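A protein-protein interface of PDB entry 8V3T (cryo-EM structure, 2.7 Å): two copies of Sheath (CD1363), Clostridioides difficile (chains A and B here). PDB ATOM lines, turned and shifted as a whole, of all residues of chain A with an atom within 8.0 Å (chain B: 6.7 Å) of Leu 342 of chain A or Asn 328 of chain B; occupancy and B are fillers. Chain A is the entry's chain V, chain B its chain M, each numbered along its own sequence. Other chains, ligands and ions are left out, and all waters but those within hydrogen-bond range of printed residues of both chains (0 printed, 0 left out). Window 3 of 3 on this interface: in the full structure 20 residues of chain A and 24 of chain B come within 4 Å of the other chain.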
ATOM      1  N   LEU A 176       7.547  12.743  18.683  1.00  0.00           N
ATOM      2  CA  LEU A 176       7.889  11.325  18.766  1.00  0.00           C
ATOM      3  C   LEU A 176       8.105  10.866  20.202  1.00  0.00           C
ATOM      4  O   LEU A 176       7.761   9.729  20.543  1.00  0.00           O
ATOM      5  CB  LEU A 176       9.142  11.032  17.941  1.00  0.00           C
ATOM      6  CG  LEU A 176       9.065  11.136  16.418  1.00  0.00           C
ATOM      7  CD1 LEU A 176       9.276  12.566  15.950  1.00  0.00           C
ATOM      8  CD2 LEU A 176      10.092  10.214  15.797  1.00  0.00           C
ATOM      9  N   SER A 177       8.682  11.718  21.049  1.00  0.00           N
ATOM     10  CA  SER A 177       9.009  11.313  22.411  1.00  0.00           C
ATOM     11  C   SER A 177       7.775  11.066  23.269  1.00  0.00           C
ATOM     12  O   SER A 177       7.868  10.350  24.271  1.00  0.00           O
ATOM     13  CB  SER A 177       9.893  12.372  23.072  1.00  0.00           C
ATOM     14  OG  SER A 177      10.359  11.929  24.335  1.00  0.00           O
ATOM     15  N   MET A 236       3.525  -5.110  21.466  1.00  0.00           N
ATOM     16  CA  MET A 236       4.199  -3.855  21.153  1.00  0.00           C
ATOM     17  C   MET A 236       3.564  -3.178  19.946  1.00  0.00           C
ATOM     18  O   MET A 236       3.461  -1.947  19.894  1.00  0.00           O
ATOM     19  CB  MET A 236       5.683  -4.118  20.901  1.00  0.00           C
ATOM     20  CG  MET A 236       6.496  -4.379  22.162  1.00  0.00           C
ATOM     21  SD  MET A 236       6.485  -3.032  23.356  1.00  0.00           S
ATOM     22  CE  MET A 236       8.128  -2.362  23.116  1.00  0.00           C
ATOM     23  N   LYS A 239       0.550  -0.337  19.831  1.00  0.00           N
ATOM     24  CA  LYS A 239       0.735   1.036  20.277  1.00  0.00           C
ATOM     25  C   LYS A 239       1.056   1.938  19.092  1.00  0.00           C
ATOM     26  O   LYS A 239       1.847   1.573  18.218  1.00  0.00           O
ATOM     27  CB  LYS A 239       1.852   1.117  21.317  1.00  0.00           C
ATOM     28  CG  LYS A 239       1.830  -0.026  22.322  1.00  0.00           C
ATOM     29  CD  LYS A 239       0.793   0.190  23.409  1.00  0.00           C
ATOM     30  CE  LYS A 239       1.142   1.381  24.282  1.00  0.00           C
ATOM     31  NZ  LYS A 239       0.341   1.396  25.536  1.00  0.00           N
ATOM     32  N   LYS A 241       2.637   4.858  19.051  1.00  0.00           N
ATOM     33  CA  LYS A 241       3.971   5.453  19.103  1.00  0.00           C
ATOM     34  C   LYS A 241       5.021   4.531  18.488  1.00  0.00           C
ATOM     35  O   LYS A 241       5.862   4.964  17.685  1.00  0.00           O
ATOM     36  CB  LYS A 241       4.305   5.772  20.561  1.00  0.00           C
ATOM     37  CG  LYS A 241       5.590   6.528  20.806  1.00  0.00           C
ATOM     38  CD  LYS A 241       5.980   6.409  22.272  1.00  0.00           C
ATOM     39  CE  LYS A 241       7.012   7.447  22.670  1.00  0.00           C
ATOM     40  NZ  LYS A 241       8.368   7.088  22.180  1.00  0.00           N
ATOM     41  N   ILE A 242       4.977   3.248  18.851  1.00  0.00           N
ATOM     42  CA  ILE A 242       5.970   2.291  18.377  1.00  0.00           C
ATOM     43  C   ILE A 242       5.846   2.087  16.873  1.00  0.00           C
ATOM     44  O   ILE A 242       6.850   2.066  16.147  1.00  0.00           O
ATOM     45  CB  ILE A 242       5.820   0.969  19.148  1.00  0.00           C
ATOM     46  CG1 ILE A 242       6.226   1.170  20.605  1.00  0.00           C
ATOM     47  CG2 ILE A 242       6.652  -0.126  18.504  1.00  0.00           C
ATOM     48  CD1 ILE A 242       5.978  -0.027  21.467  1.00  0.00           C
ATOM     49  N   THR A 245       7.354   5.172  15.067  1.00  0.00           N
ATOM     50  CA  THR A 245       8.811   5.228  14.947  1.00  0.00           C
ATOM     51  C   THR A 245       9.331   4.144  14.004  1.00  0.00           C
ATOM     52  O   THR A 245      10.287   4.377  13.248  1.00  0.00           O
ATOM     53  CB  THR A 245       9.495   5.131  16.315  1.00  0.00           C
ATOM     54  OG1 THR A 245      10.856   4.720  16.140  1.00  0.00           O
ATOM     55  CG2 THR A 245       8.808   4.137  17.206  1.00  0.00           C
ATOM     56  N   ALA A 290      18.124   9.412  20.721  1.00  0.00           N
ATOM     57  CA  ALA A 290      17.384   8.723  21.776  1.00  0.00           C
ATOM     58  C   ALA A 290      16.040   8.176  21.307  1.00  0.00           C
ATOM     59  O   ALA A 290      15.181   7.858  22.136  1.00  0.00           O
ATOM     60  CB  ALA A 290      17.182   9.621  23.003  1.00  0.00           C
ATOM     61  N   LEU A 291      15.830   8.059  19.994  1.00  0.00           N
ATOM     62  CA  LEU A 291      14.644   7.365  19.502  1.00  0.00           C
ATOM     63  C   LEU A 291      14.685   5.887  19.868  1.00  0.00           C
ATOM     64  O   LEU A 291      13.661   5.306  20.245  1.00  0.00           O
ATOM     65  CB  LEU A 291      14.515   7.533  17.989  1.00  0.00           C
ATOM     66  CG  LEU A 291      13.783   8.771  17.472  1.00  0.00           C
ATOM     67  CD1 LEU A 291      14.633  10.019  17.630  1.00  0.00           C
ATOM     68  CD2 LEU A 291      13.382   8.572  16.019  1.00  0.00           C
ATOM     69  N   ILE A 292      15.858   5.264  19.762  1.00  0.00           N
ATOM     70  CA  ILE A 292      16.037   3.852  20.062  1.00  0.00           C
ATOM     71  C   ILE A 292      17.195   3.700  21.037  1.00  0.00           C
ATOM     72  O   ILE A 292      18.034   4.590  21.190  1.00  0.00           O
ATOM     73  CB  ILE A 292      16.291   3.010  18.791  1.00  0.00           C
ATOM     74  CG1 ILE A 292      17.661   3.337  18.198  1.00  0.00           C
ATOM     75  CG2 ILE A 292      15.194   3.239  17.766  1.00  0.00           C
ATOM     76  CD1 ILE A 292      18.051   2.450  17.042  1.00  0.00           C
ATOM     77  N   GLU A 293      17.228   2.552  21.707  1.00  0.00           N
ATOM     78  CA  GLU A 293      18.302   2.266  22.644  1.00  0.00           C
ATOM     79  C   GLU A 293      19.613   1.990  21.918  1.00  0.00           C
ATOM     80  O   GLU A 293      19.656   1.752  20.709  1.00  0.00           O
ATOM     81  CB  GLU A 293      17.948   1.076  23.535  1.00  0.00           C
ATOM     82  CG  GLU A 293      16.650   1.156  24.348  1.00  0.00           C
ATOM     83  CD  GLU A 293      16.469   2.445  25.152  1.00  0.00           C
ATOM     84  OE1 GLU A 293      16.063   2.329  26.324  1.00  0.00           O
ATOM     85  OE2 GLU A 293      16.658   3.566  24.635  1.00  0.00           O
ATOM     86  N   LYS A 340      16.017  -1.877  19.667  1.00  0.00           N
ATOM     87  CA  LYS A 340      15.199  -1.925  20.872  1.00  0.00           C
ATOM     88  C   LYS A 340      14.554  -0.564  21.100  1.00  0.00           C
ATOM     89  O   LYS A 340      15.200   0.471  20.922  1.00  0.00           O
ATOM     90  CB  LYS A 340      16.033  -2.326  22.094  1.00  0.00           C
ATOM     91  CG  LYS A 340      15.213  -2.617  23.337  1.00  0.00           C
ATOM     92  CD  LYS A 340      14.473  -3.938  23.214  1.00  0.00           C
ATOM     93  CE  LYS A 340      15.439  -5.106  23.106  1.00  0.00           C
ATOM     94  NZ  LYS A 340      14.779  -6.399  23.432  1.00  0.00           N
ATOM     95  N   VAL A 341      13.279  -0.574  21.499  1.00  0.00           N
ATOM     96  CA  VAL A 341      12.488   0.639  21.689  1.00  0.00           C
ATOM     97  C   VAL A 341      11.754   0.552  23.022  1.00  0.00           C
ATOM     98  O   VAL A 341      11.301  -0.527  23.421  1.00  0.00           O
ATOM     99  CB  VAL A 341      11.484   0.852  20.533  1.00  0.00           C
ATOM    100  CG1 VAL A 341      10.743   2.168  20.695  1.00  0.00           C
ATOM    101  CG2 VAL A 341      12.194   0.811  19.189  1.00  0.00           C
ATOM    102  N   LEU A 342      11.639   1.686  23.711  1.00  0.00           N
ATOM    103  CA  LEU A 342      10.935   1.773  24.983  1.00  0.00           C
ATOM    104  C   LEU A 342       9.516   2.303  24.797  1.00  0.00           C
ATOM    105  O   LEU A 342       9.097   2.684  23.703  1.00  0.00           O
ATOM    106  CB  LEU A 342      11.686   2.672  25.968  1.00  0.00           C
ATOM    107  CG  LEU A 342      12.980   2.163  26.594  1.00  0.00           C
ATOM    108  CD1 LEU A 342      13.369   3.065  27.756  1.00  0.00           C
ATOM    109  CD2 LEU A 342      12.846   0.719  27.046  1.00  0.00           C
ATOM    110  N   ASP A 343       8.781   2.333  25.905  1.00  0.00           N
ATOM    111  CA  ASP A 343       7.407   2.810  25.955  1.00  0.00           C
ATOM    112  C   ASP A 343       7.303   3.968  26.940  1.00  0.00           C
ATOM    113  O   ASP A 343       8.203   4.213  27.747  1.00  0.00           O
ATOM    114  CB  ASP A 343       6.450   1.677  26.348  1.00  0.00           C
ATOM    115  CG  ASP A 343       5.007   1.984  26.000  1.00  0.00           C
ATOM    116  OD1 ASP A 343       4.766   2.952  25.249  1.00  0.00           O
ATOM    117  OD2 ASP A 343       4.113   1.254  26.477  1.00  0.00           O
ATOM    118  N   ALA A 344       6.189   4.689  26.864  1.00  0.00           N
ATOM    119  CA  ALA A 344       5.968   5.846  27.716  1.00  0.00           C
ATOM    120  C   ALA A 344       5.434   5.424  29.083  1.00  0.00           C
ATOM    121  O   ALA A 344       5.097   4.262  29.323  1.00  0.00           O
ATOM    122  CB  ALA A 344       5.004   6.825  27.048  1.00  0.00           C
ATOM    123  N   MET A 345       5.364   6.396  29.990  1.00  0.00           N
ATOM    124  CA  MET A 345       4.846   6.180  31.336  1.00  0.00           C
ATOM    125  C   MET A 345       3.334   6.359  31.325  1.00  0.00           C
ATOM    126  O   MET A 345       2.836   7.447  31.012  1.00  0.00           O
ATOM    127  CB  MET A 345       5.489   7.157  32.319  1.00  0.00           C
ATOM    128  CG  MET A 345       6.123   6.511  33.534  1.00  0.00           C
ATOM    129  SD  MET A 345       6.775   7.729  34.695  1.00  0.00           S
ATOM    130  CE  MET A 345       8.537   7.517  34.463  1.00  0.00           C
ATOM    131  N   THR B 266       9.467   8.870  28.569  1.00  0.00           N
ATOM    132  CA  THR B 266       9.704   7.439  28.460  1.00  0.00           C
ATOM    133  C   THR B 266       9.909   6.824  29.837  1.00  0.00           C
ATOM    134  O   THR B 266      10.438   7.459  30.754  1.00  0.00           O
ATOM    135  CB  THR B 266      10.922   7.156  27.581  1.00  0.00           C
ATOM    136  OG1 THR B 266      12.057   7.858  28.100  1.00  0.00           O
ATOM    137  CG2 THR B 266      10.665   7.609  26.156  1.00  0.00           C
ATOM    138  N   ASN B 267       9.489   5.571  29.975  1.00  0.00           N
ATOM    139  CA  ASN B 267       9.554   4.867  31.253  1.00  0.00           C
ATOM    140  C   ASN B 267      10.957   4.306  31.436  1.00  0.00           C
ATOM    141  O   ASN B 267      11.280   3.225  30.939  1.00  0.00           O
ATOM    142  CB  ASN B 267       8.503   3.764  31.310  1.00  0.00           C
ATOM    143  CG  ASN B 267       8.273   3.253  32.716  1.00  0.00           C
ATOM    144  OD1 ASN B 267       8.518   3.958  33.693  1.00  0.00           O
ATOM    145  ND2 ASN B 267       7.803   2.018  32.828  1.00  0.00           N
ATOM    146  N   SER B 268      11.798   5.043  32.159  1.00  0.00           N
ATOM    147  CA  SER B 268      13.150   4.611  32.478  1.00  0.00           C
ATOM    148  C   SER B 268      13.452   4.986  33.921  1.00  0.00           C
ATOM    149  O   SER B 268      12.723   5.757  34.550  1.00  0.00           O
ATOM    150  CB  SER B 268      14.183   5.223  31.522  1.00  0.00           C
ATOM    151  OG  SER B 268      14.091   6.635  31.503  1.00  0.00           O
ATOM    152  N   LYS B 272      11.933   7.850  36.592  1.00  0.00           N
ATOM    153  CA  LYS B 272      11.350   7.449  37.867  1.00  0.00           C
ATOM    154  C   LYS B 272      11.974   8.225  39.019  1.00  0.00           C
ATOM    155  O   LYS B 272      11.271   8.661  39.938  1.00  0.00           O
ATOM    156  CB  LYS B 272      11.527   5.945  38.074  1.00  0.00           C
ATOM    157  CG  LYS B 272      10.729   5.088  37.108  1.00  0.00           C
ATOM    158  CD  LYS B 272      10.859   3.613  37.444  1.00  0.00           C
ATOM    159  CE  LYS B 272      10.222   2.749  36.372  1.00  0.00           C
ATOM    160  NZ  LYS B 272      10.496   1.303  36.588  1.00  0.00           N
ATOM    161  N   GLN B 305       7.790  -4.563  42.441  1.00  0.00           N
ATOM    162  CA  GLN B 305       8.447  -4.650  41.143  1.00  0.00           C
ATOM    163  C   GLN B 305       9.009  -6.044  40.902  1.00  0.00           C
ATOM    164  O   GLN B 305       8.903  -6.580  39.792  1.00  0.00           O
ATOM    165  CB  GLN B 305       9.545  -3.594  41.031  1.00  0.00           C
ATOM    166  CG  GLN B 305      10.376  -3.718  39.768  1.00  0.00           C
ATOM    167  CD  GLN B 305      11.296  -2.538  39.556  1.00  0.00           C
ATOM    168  OE1 GLN B 305      11.117  -1.481  40.158  1.00  0.00           O
ATOM    169  NE2 GLN B 305      12.290  -2.712  38.696  1.00  0.00           N
ATOM    170  N   TYR B 308       6.114  -8.276  39.978  1.00  0.00           N
ATOM    171  CA  TYR B 308       5.725  -8.069  38.586  1.00  0.00           C
ATOM    172  C   TYR B 308       6.707  -8.744  37.638  1.00  0.00           C
ATOM    173  O   TYR B 308       6.304  -9.356  36.640  1.00  0.00           O
ATOM    174  CB  TYR B 308       5.626  -6.573  38.291  1.00  0.00           C
ATOM    175  CG  TYR B 308       5.416  -6.230  36.832  1.00  0.00           C
ATOM    176  CD1 TYR B 308       4.143  -6.204  36.282  1.00  0.00           C
ATOM    177  CD2 TYR B 308       6.490  -5.917  36.010  1.00  0.00           C
ATOM    178  CE1 TYR B 308       3.946  -5.886  34.952  1.00  0.00           C
ATOM    179  CE2 TYR B 308       6.304  -5.599  34.680  1.00  0.00           C
ATOM    180  CZ  TYR B 308       5.030  -5.586  34.156  1.00  0.00           C
ATOM    181  OH  TYR B 308       4.839  -5.268  32.832  1.00  0.00           O
ATOM    182  N   LEU B 309       8.005  -8.643  37.935  1.00  0.00           N
ATOM    183  CA  LEU B 309       9.010  -9.298  37.103  1.00  0.00           C
ATOM    184  C   LEU B 309       8.841 -10.813  37.121  1.00  0.00           C
ATOM    185  O   LEU B 309       8.988 -11.472  36.087  1.00  0.00           O
ATOM    186  CB  LEU B 309      10.412  -8.904  37.566  1.00  0.00           C
ATOM    187  CG  LEU B 309      10.897  -7.510  37.163  1.00  0.00           C
ATOM    188  CD1 LEU B 309      12.052  -7.071  38.045  1.00  0.00           C
ATOM    189  CD2 LEU B 309      11.299  -7.484  35.699  1.00  0.00           C
ATOM    190  N   GLU B 323      20.385  -4.651  39.287  1.00  0.00           N
ATOM    191  CA  GLU B 323      19.779  -5.122  38.048  1.00  0.00           C
ATOM    192  C   GLU B 323      18.265  -5.214  38.179  1.00  0.00           C
ATOM    193  O   GLU B 323      17.530  -4.855  37.252  1.00  0.00           O
ATOM    194  CB  GLU B 323      20.366  -6.480  37.661  1.00  0.00           C
ATOM    195  CG  GLU B 323      21.751  -6.419  37.040  1.00  0.00           C
ATOM    196  CD  GLU B 323      21.722  -6.108  35.556  1.00  0.00           C
ATOM    197  OE1 GLU B 323      20.807  -5.386  35.108  1.00  0.00           O
ATOM    198  OE2 GLU B 323      22.620  -6.589  34.834  1.00  0.00           O
ATOM    199  N   ILE B 324      17.780  -5.701  39.322  1.00  0.00           N
ATOM    200  CA  ILE B 324      16.341  -5.792  39.540  1.00  0.00           C
ATOM    201  C   ILE B 324      15.729  -4.401  39.652  1.00  0.00           C
ATOM    202  O   ILE B 324      14.662  -4.129  39.087  1.00  0.00           O
ATOM    203  CB  ILE B 324      16.046  -6.642  40.789  1.00  0.00           C
ATOM    204  CG1 ILE B 324      16.644  -8.039  40.633  1.00  0.00           C
ATOM    205  CG2 ILE B 324      14.549  -6.752  41.010  1.00  0.00           C
ATOM    206  CD1 ILE B 324      16.443  -8.922  41.843  1.00  0.00           C
ATOM    207  N   LYS B 325      16.393  -3.497  40.378  1.00  0.00           N
ATOM    208  CA  LYS B 325      15.854  -2.154  40.572  1.00  0.00           C
ATOM    209  C   LYS B 325      15.765  -1.389  39.256  1.00  0.00           C
ATOM    210  O   LYS B 325      14.782  -0.683  39.007  1.00  0.00           O
ATOM    211  CB  LYS B 325      16.712  -1.390  41.579  1.00  0.00           C
ATOM    212  CG  LYS B 325      15.937  -0.411  42.439  1.00  0.00           C
ATOM    213  CD  LYS B 325      16.837   0.245  43.470  1.00  0.00           C
ATOM    214  CE  LYS B 325      16.065   1.234  44.327  1.00  0.00           C
ATOM    215  NZ  LYS B 325      16.950   1.951  45.284  1.00  0.00           N
ATOM    216  N   GLU B 326      16.779  -1.516  38.404  1.00  0.00           N
ATOM    217  CA  GLU B 326      16.830  -0.805  37.134  1.00  0.00           C
ATOM    218  C   GLU B 326      16.184  -1.574  35.989  1.00  0.00           C
ATOM    219  O   GLU B 326      16.322  -1.165  34.833  1.00  0.00           O
ATOM    220  CB  GLU B 326      18.282  -0.475  36.770  1.00  0.00           C
ATOM    221  CG  GLU B 326      18.782   0.873  37.271  1.00  0.00           C
ATOM    222  CD  GLU B 326      19.267   0.841  38.709  1.00  0.00           C
ATOM    223  OE1 GLU B 326      18.773   0.010  39.495  1.00  0.00           O
ATOM    224  OE2 GLU B 326      20.153   1.651  39.050  1.00  0.00           O
ATOM    225  N   ALA B 327      15.498  -2.676  36.277  1.00  0.00           N
ATOM    226  CA  ALA B 327      14.889  -3.477  35.225  1.00  0.00           C
ATOM    227  C   ALA B 327      13.764  -2.712  34.537  1.00  0.00           C
ATOM    228  O   ALA B 327      13.026  -1.947  35.162  1.00  0.00           O
ATOM    229  CB  ALA B 327      14.355  -4.789  35.794  1.00  0.00           C
ATOM    230  N   ASN B 328      13.639  -2.929  33.229  1.00  0.00           N
ATOM    231  CA  ASN B 328      12.595  -2.289  32.439  1.00  0.00           C
ATOM    232  C   ASN B 328      11.275  -3.015  32.668  1.00  0.00           C
ATOM    233  O   ASN B 328      11.178  -4.225  32.442  1.00  0.00           O
ATOM    234  CB  ASN B 328      12.972  -2.295  30.960  1.00  0.00           C
ATOM    235  CG  ASN B 328      11.767  -2.185  30.049  1.00  0.00           C
ATOM    236  OD1 ASN B 328      11.262  -3.187  29.546  1.00  0.00           O
ATOM    237  ND2 ASN B 328      11.303  -0.961  29.828  1.00  0.00           N
ATOM    238  N   THR B 329      10.259  -2.278  33.112  1.00  0.00           N
ATOM    239  CA  THR B 329       8.981  -2.849  33.519  1.00  0.00           C
ATOM    240  C   THR B 329       7.829  -2.308  32.679  1.00  0.00           C
ATOM    241  O   THR B 329       6.727  -2.082  33.180  1.00  0.00           O
ATOM    242  CB  THR B 329       8.716  -2.592  35.000  1.00  0.00           C
ATOM    243  OG1 THR B 329       8.529  -1.188  35.216  1.00  0.00           O
ATOM    244  CG2 THR B 329       9.882  -3.077  35.845  1.00  0.00           C
ATOM    245  N   GLY B 330       8.068  -2.097  31.387  1.00  0.00           N
ATOM    246  CA  GLY B 330       7.014  -1.653  30.496  1.00  0.00           C
ATOM    247  C   GLY B 330       6.481  -0.271  30.809  1.00  0.00           C
ATOM    248  O   GLY B 330       7.238   0.704  30.830  1.00  0.00           O
ATOM    249  N   SER B 331       5.174  -0.171  31.046  1.00  0.00           N
ATOM    250  CA  SER B 331       4.524   1.096  31.345  1.00  0.00           C
ATOM    251  C   SER B 331       4.226   1.287  32.827  1.00  0.00           C
ATOM    252  O   SER B 331       3.603   2.288  33.192  1.00  0.00           O
ATOM    253  CB  SER B 331       3.223   1.221  30.546  1.00  0.00           C
ATOM    254  OG  SER B 331       3.465   1.751  29.256  1.00  0.00           O
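O of Ala 344 of chain A lies within hydrogen-bond range of OG of Ser 331 of chain B, at 3.0 Å. O of Asp 343 of chain A lies within hydrogen-bond range of N of Asn 267 of chain B, at 2.9 Å. The side-chain carboxylate (OD2) of Asp 343 of chain A lies within hydrogen-bond range of the side-chain hydroxyl (OG) of Ser 331 of chain B (2.9 Å).
ND2 of Asn 267 of chain B is in hydrogen-bond range of O of Gly 330 of chain B (2.5 Å). The side-chain carboxylate of Asp 343 of chain A is in salt-bridge range of the side-chain amino group of Lys 239 of chain A.
Asn 267 of chain B touches Leu 342 of chain A (O to CD1, 3.8 Å). Asn 328 of chain B touches Leu 342 of chain A. Thr 266 of chain B touches Asp 343 of chain A (CA to O, 3.6 Å). Ala 344 of chain A touches Asn 267 of chain B. CG of Met 345 of chain A touches OD1 of Asn 267 of chain B, 3.5 Å away.
Leu 342 of chain A touches just these residues of chain B: Asn 267 (3.8 Å) and Asn 328 (3.6 Å). Of the printed residues of chain B, Asp 343 of chain A touches Thr 266 (3.6 Å), Asn 267 (2.9 Å) and Ser 331 (2.9 Å). Of the printed residues of chain B, Ala 344 of chain A touches Asn 267 (3.97 Å) and Ser 331 (3.0 Å). Of the printed residues of chain B, Met 345 of chain A touches Asn 267 (3.5 Å). Of the printed residues of chain A, Asn 267 of chain B touches Leu 342 (3.8 Å), Asp 343 (2.9 Å), Ala 344 (3.97 Å) and Met 345 (3.5 Å). No residue of chain A comes within 4 Å of Ala 327 of chain B. Of chain A, only Leu 342 comes within 4 Å of Asn 328 of chain B. Of the printed residues of chain A, Ser 331 of chain B touches Asp 343 and Ala 344. The nearest printed residue of chain A that does not touch Ser 331 of chain B is Met 345 of chain A (4.5 Å).
Hydrophobic or aromatic side chains of chain A that line the printed part of chain B: Leu 342 and Met 345. Of the 16 printed residues of chain B, 4 touch a printed residue of chain A. Among the printed residues, 8 pairs touch across the chains.
No position is printed for both chains. Of the 8 pairs that touch across the chains among the printed residues, none has its exchanged pair printed and touching as well.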
